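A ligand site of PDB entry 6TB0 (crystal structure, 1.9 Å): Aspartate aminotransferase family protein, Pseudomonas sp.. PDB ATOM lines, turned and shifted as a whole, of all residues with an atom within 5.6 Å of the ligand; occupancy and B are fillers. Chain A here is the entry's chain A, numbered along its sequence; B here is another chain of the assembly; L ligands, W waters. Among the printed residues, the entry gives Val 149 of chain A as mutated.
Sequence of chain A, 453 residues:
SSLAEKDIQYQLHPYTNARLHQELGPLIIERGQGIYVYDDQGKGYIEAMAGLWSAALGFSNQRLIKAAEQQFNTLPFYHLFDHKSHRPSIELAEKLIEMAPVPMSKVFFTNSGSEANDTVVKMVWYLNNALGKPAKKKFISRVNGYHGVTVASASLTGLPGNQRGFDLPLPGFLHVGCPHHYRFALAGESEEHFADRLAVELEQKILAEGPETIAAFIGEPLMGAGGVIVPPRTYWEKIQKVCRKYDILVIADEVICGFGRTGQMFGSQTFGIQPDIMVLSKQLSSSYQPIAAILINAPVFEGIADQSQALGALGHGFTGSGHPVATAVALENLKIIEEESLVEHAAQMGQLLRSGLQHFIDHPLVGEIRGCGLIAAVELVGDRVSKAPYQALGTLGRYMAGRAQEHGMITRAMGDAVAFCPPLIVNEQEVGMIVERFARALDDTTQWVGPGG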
ATOM      1  N   TRP A  53     -20.870 -17.127  22.790  1.00  0.00           N
ATOM      2  CA  TRP A  53     -20.824 -15.771  22.201  1.00  0.00           C
ATOM      3  C   TRP A  53     -20.331 -14.777  23.247  1.00  0.00           C
ATOM      4  O   TRP A  53     -20.715 -13.603  23.158  1.00  0.00           O
ATOM      5  CB  TRP A  53     -22.205 -15.346  21.667  1.00  0.00           C
ATOM      6  CG  TRP A  53     -23.014 -16.401  20.978  1.00  0.00           C
ATOM      7  CD1 TRP A  53     -23.822 -17.344  21.551  1.00  0.00           C
ATOM      8  CD2 TRP A  53     -23.233 -16.528  19.560  1.00  0.00           C
ATOM      9  NE1 TRP A  53     -24.458 -18.085  20.585  1.00  0.00           N
ATOM     10  CE2 TRP A  53     -24.132 -17.606  19.358  1.00  0.00           C
ATOM     11  CE3 TRP A  53     -22.769 -15.848  18.441  1.00  0.00           C
ATOM     12  CZ2 TRP A  53     -24.545 -18.015  18.094  1.00  0.00           C
ATOM     13  CZ3 TRP A  53     -23.162 -16.265  17.185  1.00  0.00           C
ATOM     14  CH2 TRP A  53     -24.033 -17.339  17.018  1.00  0.00           C
ATOM     15  N   ASN A 111     -29.296 -11.806  36.700  1.00  0.00           N
ATOM     16  CA  ASN A 111     -28.269 -12.858  36.462  1.00  0.00           C
ATOM     17  C   ASN A 111     -28.129 -13.128  34.967  1.00  0.00           C
ATOM     18  O   ASN A 111     -26.994 -13.228  34.499  1.00  0.00           O
ATOM     19  CB  ASN A 111     -28.599 -14.146  37.215  1.00  0.00           C
ATOM     20  CG  ASN A 111     -28.866 -13.898  38.682  1.00  0.00           C
ATOM     21  OD1 ASN A 111     -27.954 -13.516  39.415  1.00  0.00           O
ATOM     22  ND2 ASN A 111     -30.116 -14.079  39.098  1.00  0.00           N
ATOM     23  N   SER A 112     -29.239 -13.240  34.261  1.00  0.00           N
ATOM     24  CA  SER A 112     -29.261 -13.739  32.869  1.00  0.00           C
ATOM     25  C   SER A 112     -29.876 -12.731  31.899  1.00  0.00           C
ATOM     26  O   SER A 112     -30.689 -11.873  32.314  1.00  0.00           O
ATOM     27  CB  SER A 112     -30.005 -15.056  32.818  1.00  0.00           C
ATOM     28  OG  SER A 112     -31.391 -14.882  33.036  1.00  0.00           O
ATOM     29  N   GLY A 113     -29.542 -12.887  30.614  1.00  0.00           N
ATOM     30  CA  GLY A 113     -30.221 -12.175  29.523  1.00  0.00           C
ATOM     31  C   GLY A 113     -31.700 -12.491  29.533  1.00  0.00           C
ATOM     32  O   GLY A 113     -32.522 -11.570  29.300  1.00  0.00           O
ATOM     33  N   SER A 114     -32.057 -13.753  29.757  1.00  0.00           N
ATOM     34  CA  SER A 114     -33.481 -14.183  29.779  1.00  0.00           C
ATOM     35  C   SER A 114     -34.226 -13.442  30.889  1.00  0.00           C
ATOM     36  O   SER A 114     -35.305 -12.909  30.629  1.00  0.00           O
ATOM     37  CB  SER A 114     -33.619 -15.672  29.960  1.00  0.00           C
ATOM     38  OG  SER A 114     -32.918 -16.387  28.936  1.00  0.00           O
ATOM     39  N   GLU A 115     -33.665 -13.441  32.109  1.00  0.00           N
ATOM     40  CA  GLU A 115     -34.265 -12.709  33.246  1.00  0.00           C
ATOM     41  C   GLU A 115     -34.374 -11.222  32.894  1.00  0.00           C
ATOM     42  O   GLU A 115     -35.387 -10.576  33.284  1.00  0.00           O
ATOM     43  CB  GLU A 115     -33.419 -12.795  34.498  1.00  0.00           C
ATOM     44  CG  GLU A 115     -33.479 -14.071  35.295  1.00  0.00           C
ATOM     45  CD  GLU A 115     -32.382 -14.083  36.333  1.00  0.00           C
ATOM     46  OE1 GLU A 115     -31.462 -13.223  36.208  1.00  0.00           O
ATOM     47  OE2 GLU A 115     -32.435 -14.894  37.284  1.00  0.00           O
ATOM     48  N   ASN A 117     -34.656  -9.683  29.853  1.00  0.00           N
ATOM     49  CA  ASN A 117     -35.749  -9.435  28.881  1.00  0.00           C
ATOM     50  C   ASN A 117     -37.096  -9.666  29.563  1.00  0.00           C
ATOM     51  O   ASN A 117     -38.062  -8.903  29.260  1.00  0.00           O
ATOM     52  CB  ASN A 117     -35.575 -10.237  27.589  1.00  0.00           C
ATOM     53  CG  ASN A 117     -34.507  -9.639  26.692  1.00  0.00           C
ATOM     54  OD1 ASN A 117     -34.369  -8.406  26.651  1.00  0.00           O
ATOM     55  ND2 ASN A 117     -33.814 -10.478  25.948  1.00  0.00           N
ATOM     56  N   TYR A 146     -33.539 -14.050  18.945  1.00  0.00           N
ATOM     57  CA  TYR A 146     -33.292 -14.804  20.195  1.00  0.00           C
ATOM     58  C   TYR A 146     -33.187 -13.824  21.359  1.00  0.00           C
ATOM     59  O   TYR A 146     -32.327 -12.911  21.362  1.00  0.00           O
ATOM     60  CB  TYR A 146     -32.060 -15.684  20.088  1.00  0.00           C
ATOM     61  CG  TYR A 146     -31.868 -16.579  21.282  1.00  0.00           C
ATOM     62  CD1 TYR A 146     -32.690 -17.680  21.456  1.00  0.00           C
ATOM     63  CD2 TYR A 146     -30.877 -16.354  22.221  1.00  0.00           C
ATOM     64  CE1 TYR A 146     -32.515 -18.556  22.528  1.00  0.00           C
ATOM     65  CE2 TYR A 146     -30.687 -17.203  23.298  1.00  0.00           C
ATOM     66  CZ  TYR A 146     -31.521 -18.302  23.454  1.00  0.00           C
ATOM     67  OH  TYR A 146     -31.325 -19.189  24.462  1.00  0.00           O
ATOM     68  N   HIS A 147     -34.051 -14.019  22.343  1.00  0.00           N
ATOM     69  CA  HIS A 147     -34.193 -13.100  23.504  1.00  0.00           C
ATOM     70  C   HIS A 147     -34.207 -13.895  24.814  1.00  0.00           C
ATOM     71  O   HIS A 147     -34.487 -13.312  25.871  1.00  0.00           O
ATOM     72  CB  HIS A 147     -35.424 -12.229  23.266  1.00  0.00           C
ATOM     73  CG  HIS A 147     -35.329 -11.403  22.030  1.00  0.00           C
ATOM     74  ND1 HIS A 147     -34.396 -10.382  21.897  1.00  0.00           N
ATOM     75  CD2 HIS A 147     -36.010 -11.473  20.849  1.00  0.00           C
ATOM     76  CE1 HIS A 147     -34.540  -9.837  20.701  1.00  0.00           C
ATOM     77  NE2 HIS A 147     -35.494 -10.514  20.027  1.00  0.00           N
ATOM     78  N   GLY A 148     -33.906 -15.194  24.747  1.00  0.00           N
ATOM     79  CA  GLY A 148     -33.793 -16.064  25.931  1.00  0.00           C
ATOM     80  C   GLY A 148     -34.974 -17.020  26.069  1.00  0.00           C
ATOM     81  O   GLY A 148     -35.727 -17.194  25.114  1.00  0.00           O
ATOM     82  N   VAL A 149     -35.110 -17.623  27.247  1.00  0.00           N
ATOM     83  CA  VAL A 149     -35.821 -18.926  27.414  1.00  0.00           C
ATOM     84  C   VAL A 149     -36.811 -18.923  28.581  1.00  0.00           C
ATOM     85  O   VAL A 149     -37.458 -19.972  28.771  1.00  0.00           O
ATOM     86  CB  VAL A 149     -34.800 -20.076  27.544  1.00  0.00           C
ATOM     87  CG1 VAL A 149     -33.920 -20.164  26.292  1.00  0.00           C
ATOM     88  CG2 VAL A 149     -33.990 -19.950  28.810  1.00  0.00           C
ATOM     89  N   GLU A 220     -32.410  -7.552  18.456  1.00  0.00           N
ATOM     90  CA  GLU A 220     -30.929  -7.574  18.390  1.00  0.00           C
ATOM     91  C   GLU A 220     -30.512  -6.688  17.226  1.00  0.00           C
ATOM     92  O   GLU A 220     -31.067  -6.823  16.152  1.00  0.00           O
ATOM     93  CB  GLU A 220     -30.461  -8.990  18.132  1.00  0.00           C
ATOM     94  CG  GLU A 220     -30.859 -10.010  19.174  1.00  0.00           C
ATOM     95  CD  GLU A 220     -30.770 -11.384  18.580  1.00  0.00           C
ATOM     96  OE1 GLU A 220     -29.656 -11.981  18.646  1.00  0.00           O
ATOM     97  OE2 GLU A 220     -31.788 -11.855  17.997  1.00  0.00           O
ATOM     98  N   ALA A 225     -27.887 -15.815  17.657  1.00  0.00           N
ATOM     99  CA  ALA A 225     -28.188 -17.267  17.739  1.00  0.00           C
ATOM    100  C   ALA A 225     -29.077 -17.706  16.580  1.00  0.00           C
ATOM    101  O   ALA A 225     -28.994 -18.871  16.179  1.00  0.00           O
ATOM    102  CB  ALA A 225     -28.824 -17.600  19.055  1.00  0.00           C
ATOM    103  N   ASP A 253     -31.714  -5.381  22.199  1.00  0.00           N
ATOM    104  CA  ASP A 253     -31.146  -6.569  22.869  1.00  0.00           C
ATOM    105  C   ASP A 253     -29.694  -6.695  22.421  1.00  0.00           C
ATOM    106  O   ASP A 253     -29.446  -7.216  21.312  1.00  0.00           O
ATOM    107  CB  ASP A 253     -31.943  -7.825  22.587  1.00  0.00           C
ATOM    108  CG  ASP A 253     -31.451  -9.002  23.422  1.00  0.00           C
ATOM    109  OD1 ASP A 253     -30.304  -8.925  23.922  1.00  0.00           O
ATOM    110  OD2 ASP A 253     -32.202  -9.999  23.553  1.00  0.00           O
ATOM    111  N   GLU A 254     -28.774  -6.186  23.251  1.00  0.00           N
ATOM    112  CA  GLU A 254     -27.318  -6.100  22.984  1.00  0.00           C
ATOM    113  C   GLU A 254     -26.603  -7.251  23.687  1.00  0.00           C
ATOM    114  O   GLU A 254     -25.377  -7.153  23.906  1.00  0.00           O
ATOM    115  CB  GLU A 254     -26.830  -4.716  23.448  1.00  0.00           C
ATOM    116  CG  GLU A 254     -27.331  -3.590  22.559  1.00  0.00           C
ATOM    117  CD  GLU A 254     -26.303  -3.010  21.588  1.00  0.00           C
ATOM    118  OE1 GLU A 254     -25.292  -3.704  21.295  1.00  0.00           O
ATOM    119  OE2 GLU A 254     -26.521  -1.866  21.107  1.00  0.00           O
ATOM    120  N   VAL A 255     -27.291  -8.328  24.039  1.00  0.00           N
ATOM    121  CA  VAL A 255     -26.663  -9.391  24.870  1.00  0.00           C
ATOM    122  C   VAL A 255     -25.461  -9.983  24.116  1.00  0.00           C
ATOM    123  O   VAL A 255     -24.465 -10.279  24.763  1.00  0.00           O
ATOM    124  CB  VAL A 255     -27.687 -10.444  25.319  1.00  0.00           C
ATOM    125  CG1 VAL A 255     -27.010 -11.714  25.837  1.00  0.00           C
ATOM    126  CG2 VAL A 255     -28.614  -9.871  26.385  1.00  0.00           C
ATOM    127  N   ILE A 256     -25.536 -10.138  22.799  1.00  0.00           N
ATOM    128  CA  ILE A 256     -24.356 -10.582  21.992  1.00  0.00           C
ATOM    129  C   ILE A 256     -23.617  -9.356  21.431  1.00  0.00           C
ATOM    130  O   ILE A 256     -22.358  -9.352  21.471  1.00  0.00           O
ATOM    131  CB  ILE A 256     -24.761 -11.565  20.879  1.00  0.00           C
ATOM    132  CG1 ILE A 256     -25.011 -12.968  21.467  1.00  0.00           C
ATOM    133  CG2 ILE A 256     -23.726 -11.586  19.787  1.00  0.00           C
ATOM    134  CD1 ILE A 256     -25.615 -13.968  20.462  1.00  0.00           C
ATOM    135  N   SER A 281     -25.477  -8.562  28.508  1.00  0.00           N
ATOM    136  CA  SER A 281     -24.968  -9.729  29.258  1.00  0.00           C
ATOM    137  C   SER A 281     -23.755 -10.301  28.519  1.00  0.00           C
ATOM    138  O   SER A 281     -23.073  -9.550  27.804  1.00  0.00           O
ATOM    139  CB  SER A 281     -26.080 -10.731  29.512  1.00  0.00           C
ATOM    140  OG  SER A 281     -25.724 -11.660  30.528  1.00  0.00           O
ATOM    141  N   LYS A 282     -23.463 -11.574  28.746  1.00  0.00           N
ATOM    142  CA  LYS A 282     -22.433 -12.351  28.000  1.00  0.00           C
ATOM    143  C   LYS A 282     -21.101 -11.617  28.094  1.00  0.00           C
ATOM    144  O   LYS A 282     -20.427 -11.750  29.135  1.00  0.00           O
ATOM    145  CB  LYS A 282     -22.965 -12.650  26.592  1.00  0.00           C
ATOM    146  CG  LYS A 282     -23.961 -13.799  26.546  1.00  0.00           C
ATOM    147  CD  LYS A 282     -24.346 -14.251  25.120  1.00  0.00           C
ATOM    148  CE  LYS A 282     -25.276 -15.474  25.090  1.00  0.00           C
ATOM    149  NZ  LYS A 282     -26.654 -15.110  24.655  1.00  0.00           N
ATOM    150  N   ASN B 111     -29.534 -20.064  37.038  1.00  0.00           N
ATOM    151  CA  ASN B 111     -28.856 -19.039  37.885  1.00  0.00           C
ATOM    152  C   ASN B 111     -29.706 -18.753  39.122  1.00  0.00           C
ATOM    153  O   ASN B 111     -29.141 -18.606  40.224  1.00  0.00           O
ATOM    154  CB  ASN B 111     -28.606 -17.765  37.087  1.00  0.00           C
ATOM    155  CG  ASN B 111     -27.876 -18.005  35.784  1.00  0.00           C
ATOM    156  OD1 ASN B 111     -26.703 -18.367  35.816  1.00  0.00           O
ATOM    157  ND2 ASN B 111     -28.574 -17.787  34.656  1.00  0.00           N
ATOM    158  N   GLU B 115     -35.770 -18.277  37.770  1.00  0.00           N
ATOM    159  CA  GLU B 115     -35.515 -19.020  36.519  1.00  0.00           C
ATOM    160  C   GLU B 115     -35.863 -20.504  36.725  1.00  0.00           C
ATOM    161  O   GLU B 115     -36.373 -21.133  35.776  1.00  0.00           O
ATOM    162  CB  GLU B 115     -34.062 -18.949  36.101  1.00  0.00           C
ATOM    163  CG  GLU B 115     -33.609 -17.660  35.429  1.00  0.00           C
ATOM    164  CD  GLU B 115     -32.089 -17.694  35.347  1.00  0.00           C
ATOM    165  OE1 GLU B 115     -31.491 -18.586  36.053  1.00  0.00           O
ATOM    166  OE2 GLU B 115     -31.499 -16.887  34.570  1.00  0.00           O
ATOM    167  N   GLY B 317     -32.286 -23.494  27.934  1.00  0.00           N
ATOM    168  CA  GLY B 317     -30.986 -23.350  28.585  1.00  0.00           C
ATOM    169  C   GLY B 317     -30.632 -21.897  28.769  1.00  0.00           C
ATOM    170  O   GLY B 317     -30.936 -21.093  27.880  1.00  0.00           O
ATOM    171  N   PHE B 318     -29.952 -21.614  29.878  1.00  0.00           N
ATOM    172  CA  PHE B 318     -29.354 -20.312  30.190  1.00  0.00           C
ATOM    173  C   PHE B 318     -27.859 -20.427  29.968  1.00  0.00           C
ATOM    174  O   PHE B 318     -27.278 -21.489  30.205  1.00  0.00           O
ATOM    175  CB  PHE B 318     -29.670 -19.910  31.629  1.00  0.00           C
ATOM    176  CG  PHE B 318     -31.144 -19.904  31.921  1.00  0.00           C
ATOM    177  CD1 PHE B 318     -31.928 -18.786  31.641  1.00  0.00           C
ATOM    178  CD2 PHE B 318     -31.745 -21.000  32.516  1.00  0.00           C
ATOM    179  CE1 PHE B 318     -33.280 -18.783  31.932  1.00  0.00           C
ATOM    180  CE2 PHE B 318     -33.100 -21.005  32.819  1.00  0.00           C
ATOM    181  CZ  PHE B 318     -33.880 -19.894  32.508  1.00  0.00           C
ATOM    182  N   THR B 319     -27.262 -19.342  29.487  1.00  0.00           N
ATOM    183  CA  THR B 319     -25.797 -19.241  29.318  1.00  0.00           C
ATOM    184  C   THR B 319     -25.112 -19.740  30.600  1.00  0.00           C
ATOM    185  O   THR B 319     -24.161 -20.528  30.491  1.00  0.00           O
ATOM    186  CB  THR B 319     -25.357 -17.814  28.991  1.00  0.00           C
ATOM    187  OG1 THR B 319     -25.976 -17.439  27.762  1.00  0.00           O
ATOM    188  CG2 THR B 319     -23.855 -17.691  28.855  1.00  0.00           C
ATOM    189  N   GLY B 320     -25.606 -19.315  31.762  1.00  0.00           N
ATOM    190  CA  GLY B 320     -25.013 -19.604  33.078  1.00  0.00           C
ATOM    191  C   GLY B 320     -25.400 -20.958  33.633  1.00  0.00           C
ATOM    192  O   GLY B 320     -24.927 -21.260  34.747  1.00  0.00           O
HETATM  193  N1  LIG L   1     -30.643 -12.230  24.124  1.00  0.00           N
HETATM  194  C1  LIG L   1     -29.666 -12.529  23.265  1.00  0.00           C
HETATM  195  C2  LIG L   1     -29.515 -11.706  22.031  1.00  0.00           C
HETATM  196  C3  LIG L   1     -28.774 -13.566  23.538  1.00  0.00           C
HETATM  197  O1  LIG L   1     -27.831 -13.850  22.612  1.00  0.00           O
HETATM  198  C4  LIG L   1     -28.893 -14.298  24.737  1.00  0.00           C
HETATM  199  C5  LIG L   1     -27.907 -15.331  25.034  1.00  0.00           C
HETATM  200  C6  LIG L   1     -29.975 -14.004  25.594  1.00  0.00           C
HETATM  201  C7  LIG L   1     -30.804 -12.980  25.240  1.00  0.00           C
HETATM  202  C8  LIG L   1     -30.263 -14.790  26.847  1.00  0.00           C
HETATM  203  O2  LIG L   1     -29.215 -14.760  27.859  1.00  0.00           O
HETATM  204  P1  LIG L   1     -29.128 -15.927  28.956  1.00  0.00           P
HETATM  205  O3  LIG L   1     -28.621 -17.151  28.203  1.00  0.00           O
HETATM  206  O4  LIG L   1     -30.556 -16.129  29.588  1.00  0.00           O
HETATM  207  O5  LIG L   1     -28.108 -15.391  29.950  1.00  0.00           O
HETATM  208  O   HOH W   1     -27.278 -17.001  31.997  1.00  0.00           O
HETATM  209  O   HOH W   2     -25.617 -14.333  30.148  1.00  0.00           O
HETATM  210  O   HOH W   3     -29.692 -18.924  26.563  1.00  0.00           O
HETATM  211  O   HOH W   4     -28.777 -14.327  19.967  1.00  0.00           O
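O5 of the ligand lies within hydrogen-bond range of N of Gly 113, at 3.0 Å. The backbone NH of Thr 319 of chain B sits at hydrogen-bond distance from an oxygen (O3) of the ligand (2.9 Å). The side-chain amino group (NZ) of Lys 282 is bonded to a carbon (C5) of the ligand (1.3 Å). The side-chain hydroxyl (OG) of Ser 114 lies within hydrogen-bond range of an oxygen (O4) of the ligand (2.5 Å). OG1 of Thr 319 of chain B lies within hydrogen-bond range of O3 of the ligand, at 2.7 Å. The side-chain carboxylate (OD2) of Asp 253 sits at hydrogen-bond distance from a nitrogen (N1) of the ligand (2.8 Å). An oxygen (O4) of the ligand lies within hydrogen-bond range of the backbone NH of Ser 114, at 2.8 Å.
The side-chain hydroxyl (OG) of Ser 114 sits at hydrogen-bond distance from the backbone NH (N) of Val 149 (3.0 Å). The backbone NH (N) of Val 255 lies within hydrogen-bond range of the side-chain carboxylate (OD1) of Asp 253, 3.1 Å away. The backbone NH (N) of Glu 115 of chain A is in hydrogen-bond range of the side-chain hydroxyl (OG) of Ser 112 (2.8 Å). The side-chain amide nitrogen (ND2) of Asn 117 sits at hydrogen-bond distance from the side-chain carboxylate (OD2) of Asp 253 (2.9 Å). The backbone carbonyl oxygen (O) of His 147 is in hydrogen-bond range of the side-chain amide nitrogen (ND2) of Asn 117 (2.9 Å). The backbone NH of Tyr 146 is in hydrogen-bond range of the side-chain carboxylate of Glu 220, at 3.0 Å. OD2 of Asp 253 lies within hydrogen-bond range of ND1 of His 147. The side-chain carboxylate (OE2) of Glu 115 of chain B is in hydrogen-bond range of the side-chain hydroxyl (OG) of Ser 112.
O of Tyr 146 sits close to N1 of the ligand, 3.3 Å away. Ser 112 touches the ligand. Asn 117 touches the ligand (ND2 to C7, 3.98 Å). C of His 147 touches C7 of the ligand, at 3.5 Å. Gly 148 touches the ligand (N to C7, 3.8 Å). OE1 of Glu 220 touches C2 of the ligand (3.4 Å). CG1 of Val 255 touches C4 of the ligand, at 3.4 Å. CD1 of Ile 256 touches O1 of the ligand (3.1 Å). Phe 318 of chain B touches the ligand (CD1 to O4, 3.6 Å). Hydrophobic or aromatic side chains that line the ligand: Tyr 146, Val 255, Ile 256 and Phe 318 of chain B. Within 4 Å of the ligand: Ser 112, Gly 113, Ser 114, Asn 117, Tyr 146, His 147, Gly 148, Glu 220, Asp 253, Val 255, Ile 256, Lys 282, Phe 318 of chain B and Thr 319 of chain B.
Water W3 lies within hydrogen-bond range of an oxygen (O3) of the ligand (2.6 Å), the side-chain hydroxyl (OH) of Tyr 146 (2.7 Å) and the backbone carbonyl oxygen (O) of Gly 317 of chain B (2.8 Å). Water W2 lies within hydrogen-bond range of the side-chain hydroxyl (OG) of Ser 281 (2.7 Å) and an oxygen (O5) of the ligand (2.7 Å). Water W4 lies within hydrogen-bond range of OE1 of Glu 220 (2.8 Å), O1 of the ligand (2.8 Å) and N of Ala 225 (2.9 Å).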
